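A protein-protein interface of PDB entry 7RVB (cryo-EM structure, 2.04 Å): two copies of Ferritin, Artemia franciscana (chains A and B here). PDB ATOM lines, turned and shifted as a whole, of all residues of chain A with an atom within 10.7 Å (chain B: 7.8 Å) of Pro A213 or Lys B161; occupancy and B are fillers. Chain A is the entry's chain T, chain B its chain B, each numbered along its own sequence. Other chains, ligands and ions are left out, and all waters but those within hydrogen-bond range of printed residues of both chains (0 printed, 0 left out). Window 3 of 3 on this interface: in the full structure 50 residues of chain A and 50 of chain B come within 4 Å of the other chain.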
ATOM      1  N   LEU A 203     -13.486   6.368  34.358  1.00  0.00           N
ATOM      2  CA  LEU A 203     -13.011   7.665  33.905  1.00  0.00           C
ATOM      3  C   LEU A 203     -14.116   8.703  34.046  1.00  0.00           C
ATOM      4  O   LEU A 203     -15.304   8.373  34.032  1.00  0.00           O
ATOM      5  CB  LEU A 203     -12.543   7.605  32.449  1.00  0.00           C
ATOM      6  CG  LEU A 203     -11.521   6.530  32.082  1.00  0.00           C
ATOM      7  CD1 LEU A 203     -11.415   6.390  30.577  1.00  0.00           C
ATOM      8  CD2 LEU A 203     -10.169   6.849  32.681  1.00  0.00           C
ATOM      9  N   SER A 204     -13.718   9.966  34.182  1.00  0.00           N
ATOM     10  CA  SER A 204     -14.665  11.058  34.354  1.00  0.00           C
ATOM     11  C   SER A 204     -14.052  12.337  33.796  1.00  0.00           C
ATOM     12  O   SER A 204     -12.904  12.353  33.345  1.00  0.00           O
ATOM     13  CB  SER A 204     -15.050  11.224  35.826  1.00  0.00           C
ATOM     14  OG  SER A 204     -13.994  11.807  36.564  1.00  0.00           O
ATOM     15  N   THR A 205     -14.831  13.416  33.827  1.00  0.00           N
ATOM     16  CA  THR A 205     -14.375  14.718  33.362  1.00  0.00           C
ATOM     17  C   THR A 205     -14.012  15.660  34.503  1.00  0.00           C
ATOM     18  O   THR A 205     -13.839  16.859  34.269  1.00  0.00           O
ATOM     19  CB  THR A 205     -15.432  15.378  32.472  1.00  0.00           C
ATOM     20  OG1 THR A 205     -16.681  15.438  33.170  1.00  0.00           O
ATOM     21  CG2 THR A 205     -15.614  14.593  31.185  1.00  0.00           C
ATOM     22  N   SER A 206     -13.908  15.156  35.729  1.00  0.00           N
ATOM     23  CA  SER A 206     -13.450  15.983  36.835  1.00  0.00           C
ATOM     24  C   SER A 206     -11.995  16.383  36.626  1.00  0.00           C
ATOM     25  O   SER A 206     -11.184  15.595  36.133  1.00  0.00           O
ATOM     26  CB  SER A 206     -13.604  15.238  38.159  1.00  0.00           C
ATOM     27  OG  SER A 206     -14.925  14.757  38.320  1.00  0.00           O
ATOM     28  N   ASP A 207     -11.669  17.618  37.009  1.00  0.00           N
ATOM     29  CA  ASP A 207     -10.335  18.188  36.819  1.00  0.00           C
ATOM     30  C   ASP A 207      -9.922  18.112  35.348  1.00  0.00           C
ATOM     31  O   ASP A 207      -8.910  17.512  34.985  1.00  0.00           O
ATOM     32  CB  ASP A 207      -9.308  17.497  37.720  1.00  0.00           C
ATOM     33  CG  ASP A 207      -9.565  17.745  39.191  1.00  0.00           C
ATOM     34  OD1 ASP A 207     -10.061  18.838  39.533  1.00  0.00           O
ATOM     35  OD2 ASP A 207      -9.274  16.845  40.005  1.00  0.00           O
ATOM     36  N   LEU A 208     -10.740  18.738  34.502  1.00  0.00           N
ATOM     37  CA  LEU A 208     -10.510  18.686  33.063  1.00  0.00           C
ATOM     38  C   LEU A 208      -9.186  19.336  32.687  1.00  0.00           C
ATOM     39  O   LEU A 208      -8.469  18.839  31.811  1.00  0.00           O
ATOM     40  CB  LEU A 208     -11.665  19.362  32.328  1.00  0.00           C
ATOM     41  CG  LEU A 208     -12.085  18.772  30.983  1.00  0.00           C
ATOM     42  CD1 LEU A 208     -11.877  17.270  30.959  1.00  0.00           C
ATOM     43  CD2 LEU A 208     -13.530  19.119  30.687  1.00  0.00           C
ATOM     44  N   GLU A 209      -8.843  20.447  33.336  1.00  0.00           N
ATOM     45  CA  GLU A 209      -7.631  21.180  32.991  1.00  0.00           C
ATOM     46  C   GLU A 209      -6.357  20.424  33.343  1.00  0.00           C
ATOM     47  O   GLU A 209      -5.281  20.819  32.883  1.00  0.00           O
ATOM     48  CB  GLU A 209      -7.628  22.543  33.685  1.00  0.00           C
ATOM     49  CG  GLU A 209      -7.644  22.470  35.202  1.00  0.00           C
ATOM     50  CD  GLU A 209      -9.042  22.558  35.779  1.00  0.00           C
ATOM     51  OE1 GLU A 209      -9.996  22.141  35.094  1.00  0.00           O
ATOM     52  OE2 GLU A 209      -9.185  23.043  36.920  1.00  0.00           O
ATOM     53  N   SER A 210      -6.444  19.356  34.133  1.00  0.00           N
ATOM     54  CA  SER A 210      -5.259  18.611  34.538  1.00  0.00           C
ATOM     55  C   SER A 210      -4.937  17.446  33.611  1.00  0.00           C
ATOM     56  O   SER A 210      -3.761  17.113  33.440  1.00  0.00           O
ATOM     57  CB  SER A 210      -5.426  18.090  35.967  1.00  0.00           C
ATOM     58  OG  SER A 210      -5.336  19.145  36.905  1.00  0.00           O
ATOM     59  N   ASN A 211      -5.946  16.816  33.015  1.00  0.00           N
ATOM     60  CA  ASN A 211      -5.758  15.681  32.113  1.00  0.00           C
ATOM     61  C   ASN A 211      -6.253  16.103  30.734  1.00  0.00           C
ATOM     62  O   ASN A 211      -7.394  15.820  30.365  1.00  0.00           O
ATOM     63  CB  ASN A 211      -6.504  14.454  32.618  1.00  0.00           C
ATOM     64  CG  ASN A 211      -6.660  14.443  34.123  1.00  0.00           C
ATOM     65  OD1 ASN A 211      -7.747  14.673  34.647  1.00  0.00           O
ATOM     66  ND2 ASN A 211      -5.571  14.171  34.828  1.00  0.00           N
ATOM     67  N   ILE A 212      -5.391  16.761  29.966  1.00  0.00           N
ATOM     68  CA  ILE A 212      -5.838  17.440  28.752  1.00  0.00           C
ATOM     69  C   ILE A 212      -6.129  16.450  27.630  1.00  0.00           C
ATOM     70  O   ILE A 212      -7.261  16.443  27.125  1.00  0.00           O
ATOM     71  CB  ILE A 212      -4.835  18.514  28.306  1.00  0.00           C
ATOM     72  CG1 ILE A 212      -4.699  19.580  29.391  1.00  0.00           C
ATOM     73  CG2 ILE A 212      -5.272  19.117  26.989  1.00  0.00           C
ATOM     74  CD1 ILE A 212      -5.962  20.378  29.615  1.00  0.00           C
ATOM     75  N   PRO A 213      -5.173  15.610  27.174  1.00  0.00           N
ATOM     76  CA  PRO A 213      -5.548  14.604  26.172  1.00  0.00           C
ATOM     77  C   PRO A 213      -6.527  13.609  26.770  1.00  0.00           C
ATOM     78  O   PRO A 213      -7.647  13.450  26.278  1.00  0.00           O
ATOM     79  CB  PRO A 213      -4.213  13.949  25.795  1.00  0.00           C
ATOM     80  CG  PRO A 213      -3.160  14.839  26.361  1.00  0.00           C
ATOM     81  CD  PRO A 213      -3.767  15.444  27.576  1.00  0.00           C
ATOM     82  N   ASN A 214      -6.109  12.966  27.854  1.00  0.00           N
ATOM     83  CA  ASN A 214      -6.956  12.122  28.691  1.00  0.00           C
ATOM     84  C   ASN A 214      -6.131  11.740  29.914  1.00  0.00           C
ATOM     85  O   ASN A 214      -4.940  12.051  30.002  1.00  0.00           O
ATOM     86  CB  ASN A 214      -7.476  10.888  27.947  1.00  0.00           C
ATOM     87  CG  ASN A 214      -6.367  10.037  27.381  1.00  0.00           C
ATOM     88  OD1 ASN A 214      -5.805   9.193  28.074  1.00  0.00           O
ATOM     89  ND2 ASN A 214      -6.054  10.239  26.109  1.00  0.00           N
ATOM     90  N   GLU A 215      -6.773  11.055  30.857  1.00  0.00           N
ATOM     91  CA  GLU A 215      -6.133  10.777  32.138  1.00  0.00           C
ATOM     92  C   GLU A 215      -5.066   9.692  32.033  1.00  0.00           C
ATOM     93  O   GLU A 215      -4.031   9.773  32.702  1.00  0.00           O
ATOM     94  CB  GLU A 215      -7.188  10.384  33.169  1.00  0.00           C
ATOM     95  CG  GLU A 215      -6.628  10.051  34.537  1.00  0.00           C
ATOM     96  CD  GLU A 215      -7.692   9.565  35.498  1.00  0.00           C
ATOM     97  OE1 GLU A 215      -8.882   9.566  35.118  1.00  0.00           O
ATOM     98  OE2 GLU A 215      -7.341   9.183  36.632  1.00  0.00           O
ATOM     99  N   LEU A 216      -5.293   8.671  31.207  1.00  0.00           N
ATOM    100  CA  LEU A 216      -4.410   7.510  31.208  1.00  0.00           C
ATOM    101  C   LEU A 216      -3.090   7.763  30.489  1.00  0.00           C
ATOM    102  O   LEU A 216      -2.068   7.180  30.868  1.00  0.00           O
ATOM    103  CB  LEU A 216      -5.121   6.315  30.576  1.00  0.00           C
ATOM    104  CG  LEU A 216      -6.309   5.760  31.360  1.00  0.00           C
ATOM    105  CD1 LEU A 216      -6.975   4.637  30.595  1.00  0.00           C
ATOM    106  CD2 LEU A 216      -5.867   5.288  32.730  1.00  0.00           C
ATOM    107  N   PHE A 217      -3.081   8.629  29.475  1.00  0.00           N
ATOM    108  CA  PHE A 217      -1.939   8.718  28.571  1.00  0.00           C
ATOM    109  C   PHE A 217      -0.650   9.143  29.264  1.00  0.00           C
ATOM    110  O   PHE A 217       0.432   8.904  28.720  1.00  0.00           O
ATOM    111  CB  PHE A 217      -2.245   9.681  27.426  1.00  0.00           C
ATOM    112  CG  PHE A 217      -2.801   9.011  26.205  1.00  0.00           C
ATOM    113  CD1 PHE A 217      -3.485   7.815  26.307  1.00  0.00           C
ATOM    114  CD2 PHE A 217      -2.633   9.575  24.955  1.00  0.00           C
ATOM    115  CE1 PHE A 217      -3.996   7.198  25.186  1.00  0.00           C
ATOM    116  CE2 PHE A 217      -3.141   8.960  23.830  1.00  0.00           C
ATOM    117  CZ  PHE A 217      -3.823   7.771  23.946  1.00  0.00           C
ATOM    118  N   ASP A 218      -0.724   9.764  30.438  1.00  0.00           N
ATOM    119  CA  ASP A 218       0.476  10.207  31.134  1.00  0.00           C
ATOM    120  C   ASP A 218       0.881   9.285  32.278  1.00  0.00           C
ATOM    121  O   ASP A 218       1.764   9.648  33.064  1.00  0.00           O
ATOM    122  CB  ASP A 218       0.298  11.639  31.645  1.00  0.00           C
ATOM    123  CG  ASP A 218      -0.922  11.804  32.521  1.00  0.00           C
ATOM    124  OD1 ASP A 218      -1.475  10.790  32.989  1.00  0.00           O
ATOM    125  OD2 ASP A 218      -1.328  12.962  32.747  1.00  0.00           O
ATOM    126  N   ALA A 219       0.274   8.098  32.375  1.00  0.00           N
ATOM    127  CA  ALA A 219       0.537   7.208  33.504  1.00  0.00           C
ATOM    128  C   ALA A 219       2.028   6.961  33.694  1.00  0.00           C
ATOM    129  O   ALA A 219       2.556   7.113  34.803  1.00  0.00           O
ATOM    130  CB  ALA A 219      -0.205   5.886  33.309  1.00  0.00           C
ATOM    131  N   VAL B 120     -16.331   2.574  19.610  1.00  0.00           N
ATOM    132  CA  VAL B 120     -16.742   3.969  19.458  1.00  0.00           C
ATOM    133  C   VAL B 120     -18.198   4.058  19.009  1.00  0.00           C
ATOM    134  O   VAL B 120     -18.980   4.875  19.525  1.00  0.00           O
ATOM    135  CB  VAL B 120     -15.800   4.697  18.483  1.00  0.00           C
ATOM    136  CG1 VAL B 120     -16.393   6.024  18.056  1.00  0.00           C
ATOM    137  CG2 VAL B 120     -14.442   4.907  19.120  1.00  0.00           C
ATOM    138  N   LYS B 123     -20.486   3.366  21.900  1.00  0.00           N
ATOM    139  CA  LYS B 123     -20.578   4.515  22.798  1.00  0.00           C
ATOM    140  C   LYS B 123     -21.530   5.570  22.248  1.00  0.00           C
ATOM    141  O   LYS B 123     -22.319   6.161  22.999  1.00  0.00           O
ATOM    142  CB  LYS B 123     -19.192   5.113  23.031  1.00  0.00           C
ATOM    143  CG  LYS B 123     -18.254   4.225  23.823  1.00  0.00           C
ATOM    144  CD  LYS B 123     -18.729   4.054  25.248  1.00  0.00           C
ATOM    145  CE  LYS B 123     -17.860   3.068  26.002  1.00  0.00           C
ATOM    146  NZ  LYS B 123     -17.687   1.800  25.250  1.00  0.00           N
ATOM    147  N   GLU B 155     -19.195   9.324  32.216  1.00  0.00           N
ATOM    148  CA  GLU B 155     -18.372   8.162  31.899  1.00  0.00           C
ATOM    149  C   GLU B 155     -18.302   7.936  30.399  1.00  0.00           C
ATOM    150  O   GLU B 155     -17.228   7.662  29.853  1.00  0.00           O
ATOM    151  CB  GLU B 155     -18.942   6.923  32.586  1.00  0.00           C
ATOM    152  CG  GLU B 155     -18.330   6.584  33.922  1.00  0.00           C
ATOM    153  CD  GLU B 155     -19.023   5.407  34.584  1.00  0.00           C
ATOM    154  OE1 GLU B 155     -18.326   4.500  35.078  1.00  0.00           O
ATOM    155  OE2 GLU B 155     -20.270   5.391  34.613  1.00  0.00           O
ATOM    156  N   VAL B 156     -19.444   8.044  29.720  1.00  0.00           N
ATOM    157  CA  VAL B 156     -19.489   7.797  28.284  1.00  0.00           C
ATOM    158  C   VAL B 156     -18.644   8.820  27.542  1.00  0.00           C
ATOM    159  O   VAL B 156     -17.890   8.473  26.625  1.00  0.00           O
ATOM    160  CB  VAL B 156     -20.946   7.793  27.791  1.00  0.00           C
ATOM    161  CG1 VAL B 156     -21.004   7.498  26.311  1.00  0.00           C
ATOM    162  CG2 VAL B 156     -21.755   6.777  28.566  1.00  0.00           C
ATOM    163  N   ILE B 157     -18.742  10.094  27.929  1.00  0.00           N
ATOM    164  CA  ILE B 157     -17.962  11.131  27.255  1.00  0.00           C
ATOM    165  C   ILE B 157     -16.467  10.871  27.420  1.00  0.00           C
ATOM    166  O   ILE B 157     -15.690  10.919  26.451  1.00  0.00           O
ATOM    167  CB  ILE B 157     -18.355  12.523  27.780  1.00  0.00           C
ATOM    168  CG1 ILE B 157     -19.848  12.779  27.561  1.00  0.00           C
ATOM    169  CG2 ILE B 157     -17.523  13.604  27.118  1.00  0.00           C
ATOM    170  CD1 ILE B 157     -20.209  13.156  26.155  1.00  0.00           C
ATOM    171  N   ALA B 158     -16.041  10.575  28.653  1.00  0.00           N
ATOM    172  CA  ALA B 158     -14.618  10.346  28.899  1.00  0.00           C
ATOM    173  C   ALA B 158     -14.105   9.127  28.140  1.00  0.00           C
ATOM    174  O   ALA B 158     -13.024   9.168  27.529  1.00  0.00           O
ATOM    175  CB  ALA B 158     -14.368  10.195  30.398  1.00  0.00           C
ATOM    176  N   TRP B 159     -14.868   8.031  28.159  1.00  0.00           N
ATOM    177  CA  TRP B 159     -14.446   6.824  27.457  1.00  0.00           C
ATOM    178  C   TRP B 159     -14.377   7.055  25.955  1.00  0.00           C
ATOM    179  O   TRP B 159     -13.477   6.539  25.282  1.00  0.00           O
ATOM    180  CB  TRP B 159     -15.389   5.668  27.785  1.00  0.00           C
ATOM    181  CG  TRP B 159     -14.989   4.909  29.007  1.00  0.00           C
ATOM    182  CD1 TRP B 159     -15.287   5.221  30.297  1.00  0.00           C
ATOM    183  CD2 TRP B 159     -14.210   3.711  29.054  1.00  0.00           C
ATOM    184  NE1 TRP B 159     -14.744   4.293  31.146  1.00  0.00           N
ATOM    185  CE2 TRP B 159     -14.078   3.354  30.407  1.00  0.00           C
ATOM    186  CE3 TRP B 159     -13.614   2.904  28.082  1.00  0.00           C
ATOM    187  CZ2 TRP B 159     -13.375   2.226  30.814  1.00  0.00           C
ATOM    188  CZ3 TRP B 159     -12.917   1.786  28.488  1.00  0.00           C
ATOM    189  CH2 TRP B 159     -12.802   1.456  29.840  1.00  0.00           C
ATOM    190  N   ASN B 160     -15.323   7.821  25.408  1.00  0.00           N
ATOM    191  CA  ASN B 160     -15.292   8.118  23.982  1.00  0.00           C
ATOM    192  C   ASN B 160     -14.035   8.891  23.610  1.00  0.00           C
ATOM    193  O   ASN B 160     -13.388   8.587  22.599  1.00  0.00           O
ATOM    194  CB  ASN B 160     -16.542   8.898  23.585  1.00  0.00           C
ATOM    195  CG  ASN B 160     -16.599   9.184  22.104  1.00  0.00           C
ATOM    196  OD1 ASN B 160     -16.898   8.302  21.303  1.00  0.00           O
ATOM    197  ND2 ASN B 160     -16.311  10.421  21.730  1.00  0.00           N
ATOM    198  N   LYS B 161     -13.663   9.885  24.421  1.00  0.00           N
ATOM    199  CA  LYS B 161     -12.434  10.623  24.133  1.00  0.00           C
ATOM    200  C   LYS B 161     -11.213   9.708  24.172  1.00  0.00           C
ATOM    201  O   LYS B 161     -10.352   9.766  23.280  1.00  0.00           O
ATOM    202  CB  LYS B 161     -12.266  11.781  25.116  1.00  0.00           C
ATOM    203  CG  LYS B 161     -11.015  12.619  24.892  1.00  0.00           C
ATOM    204  CD  LYS B 161     -10.893  13.064  23.445  1.00  0.00           C
ATOM    205  CE  LYS B 161     -10.163  14.388  23.322  1.00  0.00           C
ATOM    206  NZ  LYS B 161      -8.689  14.239  23.386  1.00  0.00           N
ATOM    207  N   PHE B 162     -11.127   8.848  25.190  1.00  0.00           N
ATOM    208  CA  PHE B 162      -9.978   7.950  25.300  1.00  0.00           C
ATOM    209  C   PHE B 162      -9.883   7.010  24.101  1.00  0.00           C
ATOM    210  O   PHE B 162      -8.800   6.824  23.523  1.00  0.00           O
ATOM    211  CB  PHE B 162     -10.065   7.158  26.604  1.00  0.00           C
ATOM    212  CG  PHE B 162      -9.078   6.032  26.701  1.00  0.00           C
ATOM    213  CD1 PHE B 162      -7.727   6.285  26.836  1.00  0.00           C
ATOM    214  CD2 PHE B 162      -9.506   4.719  26.667  1.00  0.00           C
ATOM    215  CE1 PHE B 162      -6.823   5.250  26.929  1.00  0.00           C
ATOM    216  CE2 PHE B 162      -8.605   3.682  26.759  1.00  0.00           C
ATOM    217  CZ  PHE B 162      -7.262   3.947  26.890  1.00  0.00           C
ATOM    218  N   LEU B 163     -11.010   6.417  23.701  1.00  0.00           N
ATOM    219  CA  LEU B 163     -10.995   5.484  22.582  1.00  0.00           C
ATOM    220  C   LEU B 163     -10.654   6.186  21.273  1.00  0.00           C
ATOM    221  O   LEU B 163      -9.948   5.624  20.431  1.00  0.00           O
ATOM    222  CB  LEU B 163     -12.339   4.767  22.476  1.00  0.00           C
ATOM    223  CG  LEU B 163     -12.670   3.799  23.614  1.00  0.00           C
ATOM    224  CD1 LEU B 163     -14.099   3.309  23.503  1.00  0.00           C
ATOM    225  CD2 LEU B 163     -11.706   2.631  23.635  1.00  0.00           C
ATOM    226  N   SER B 164     -11.147   7.413  21.081  1.00  0.00           N
ATOM    227  CA  SER B 164     -10.804   8.155  19.871  1.00  0.00           C
ATOM    228  C   SER B 164      -9.311   8.456  19.809  1.00  0.00           C
ATOM    229  O   SER B 164      -8.694   8.356  18.739  1.00  0.00           O
ATOM    230  CB  SER B 164     -11.614   9.447  19.802  1.00  0.00           C
ATOM    231  OG  SER B 164     -12.950   9.184  19.424  1.00  0.00           O
ATOM    232  N   ASP B 165      -8.714   8.833  20.943  1.00  0.00           N
ATOM    233  CA  ASP B 165      -7.273   9.069  20.962  1.00  0.00           C
ATOM    234  C   ASP B 165      -6.501   7.803  20.604  1.00  0.00           C
ATOM    235  O   ASP B 165      -5.553   7.844  19.803  1.00  0.00           O
ATOM    236  CB  ASP B 165      -6.841   9.582  22.334  1.00  0.00           C
ATOM    237  CG  ASP B 165      -7.260  11.014  22.578  1.00  0.00           C
ATOM    238  OD1 ASP B 165      -7.668  11.691  21.613  1.00  0.00           O
ATOM    239  OD2 ASP B 165      -7.181  11.465  23.738  1.00  0.00           O
ATOM    240  N   CYS B 166      -6.901   6.666  21.180  1.00  0.00           N
ATOM    241  CA  CYS B 166      -6.233   5.408  20.856  1.00  0.00           C
ATOM    242  C   CYS B 166      -6.364   5.076  19.375  1.00  0.00           C
ATOM    243  O   CYS B 166      -5.404   4.620  18.744  1.00  0.00           O
ATOM    244  CB  CYS B 166      -6.801   4.273  21.709  1.00  0.00           C
ATOM    245  SG  CYS B 166      -6.115   4.157  23.370  1.00  0.00           S
ATOM    246  N   LEU B 167      -7.550   5.297  18.803  1.00  0.00           N
ATOM    247  CA  LEU B 167      -7.766   5.003  17.391  1.00  0.00           C
ATOM    248  C   LEU B 167      -6.891   5.872  16.497  1.00  0.00           C
ATOM    249  O   LEU B 167      -6.323   5.386  15.511  1.00  0.00           O
ATOM    250  CB  LEU B 167      -9.241   5.189  17.043  1.00  0.00           C
ATOM    251  CG  LEU B 167      -9.685   4.795  15.638  1.00  0.00           C
ATOM    252  CD1 LEU B 167      -9.254   3.380  15.320  1.00  0.00           C
ATOM    253  CD2 LEU B 167     -11.187   4.934  15.510  1.00  0.00           C
ATOM    254  N   SER B 168      -6.778   7.163  16.815  1.00  0.00           N
ATOM    255  CA  SER B 168      -5.913   8.035  16.024  1.00  0.00           C
ATOM    256  C   SER B 168      -4.460   7.585  16.100  1.00  0.00           C
ATOM    257  O   SER B 168      -3.754   7.552  15.081  1.00  0.00           O
ATOM    258  CB  SER B 168      -6.046   9.483  16.491  1.00  0.00           C
ATOM    259  OG  SER B 168      -7.386   9.925  16.396  1.00  0.00           O
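No position is printed for both chains.
Of the printed residues of chain B, Ser A204 touches Ala B158.
Thr A205 touches none of the printed residues of chain B.
Leu A208 touches none of the printed residues of chain B.
Of the printed residues of chain B, Asn A214 touches Phe B162 and Asp B165.
Printed residues of chain B within 4 Å of Leu A216: Phe B162.
Of the printed residues of chain B, Phe A217 touches Phe B162 and Asp B165.
Ala B158 touches just these residues of chain A: Leu A203 (3.8 Å) and Ser A204 (3.8 Å).
Lys B161 touches just one residue of chain A: Pro A213 (3.2 Å).
Printed residues of chain A within 4 Å of Phe B162: Asn A214 (3.7 Å), Leu A216 (3.7 Å) and Phe A217 (3.9 Å).
The nearest residue of chain A that does not touch Lys B161 is Ile A212 (4.6 Å).
The nearest printed residue of chain B that does not touch Asn A214 is Lys B161 (5.0 Å).
OD2 of Asp B165 is in salt-bridge range of NZ of Lys B161 (3.2 Å).
The backbone carbonyl oxygen (O) of Phe B162 sits close to the side-chain sulfur (SG) of Cys B166 (3.8 Å).
The backbone NH of Ser A206 lies close to the side-chain hydroxyl of Ser A204 (3.5 Å).
The side-chain amide oxygen (OD1) of Asn A214 is in hydrogen-bond range of the backbone NH (N) of Leu A216 (3.2 Å).
OD1 of Asn A214 is in hydrogen-bond range of N of Phe A217.
Printed residues of chain A that touch a printed residue of chain B: Leu A203, Ser A204, Pro A213, Asn A214, Leu A216 and Phe A217.
Among the printed residues, 11 pairs touch across the chains.
Among the printed residues, no Asp or Glu carboxylate lies within 4 Å of a Lys or Arg side-chain nitrogen of the other chain.
Among the printed residues, merely in contact across the chains: Leu A203 with Glu B155 (3.5 Å), Asn A214 with Phe B162 (3.7 Å), Leu A216 with Phe B162 (3.7 Å), Leu A203 with Ala B158 (3.8 Å), Ser A204 with Ala B158 (3.8 Å), Phe A217 with Phe B162 (3.9 Å), Phe A217 with Asp B165 (3.9 Å) and Leu A203 with Trp B159 (3.98 Å).
O of Pro A213 lies within hydrogen-bond range of NZ of Lys B161.
The side-chain carboxylate of Asp B165 sits at hydrogen-bond distance from the side-chain amide nitrogen of Asn A214 (2.9 Å).
O of Pro A213 lies close to OD2 of Asp B165, at 3.3 Å.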
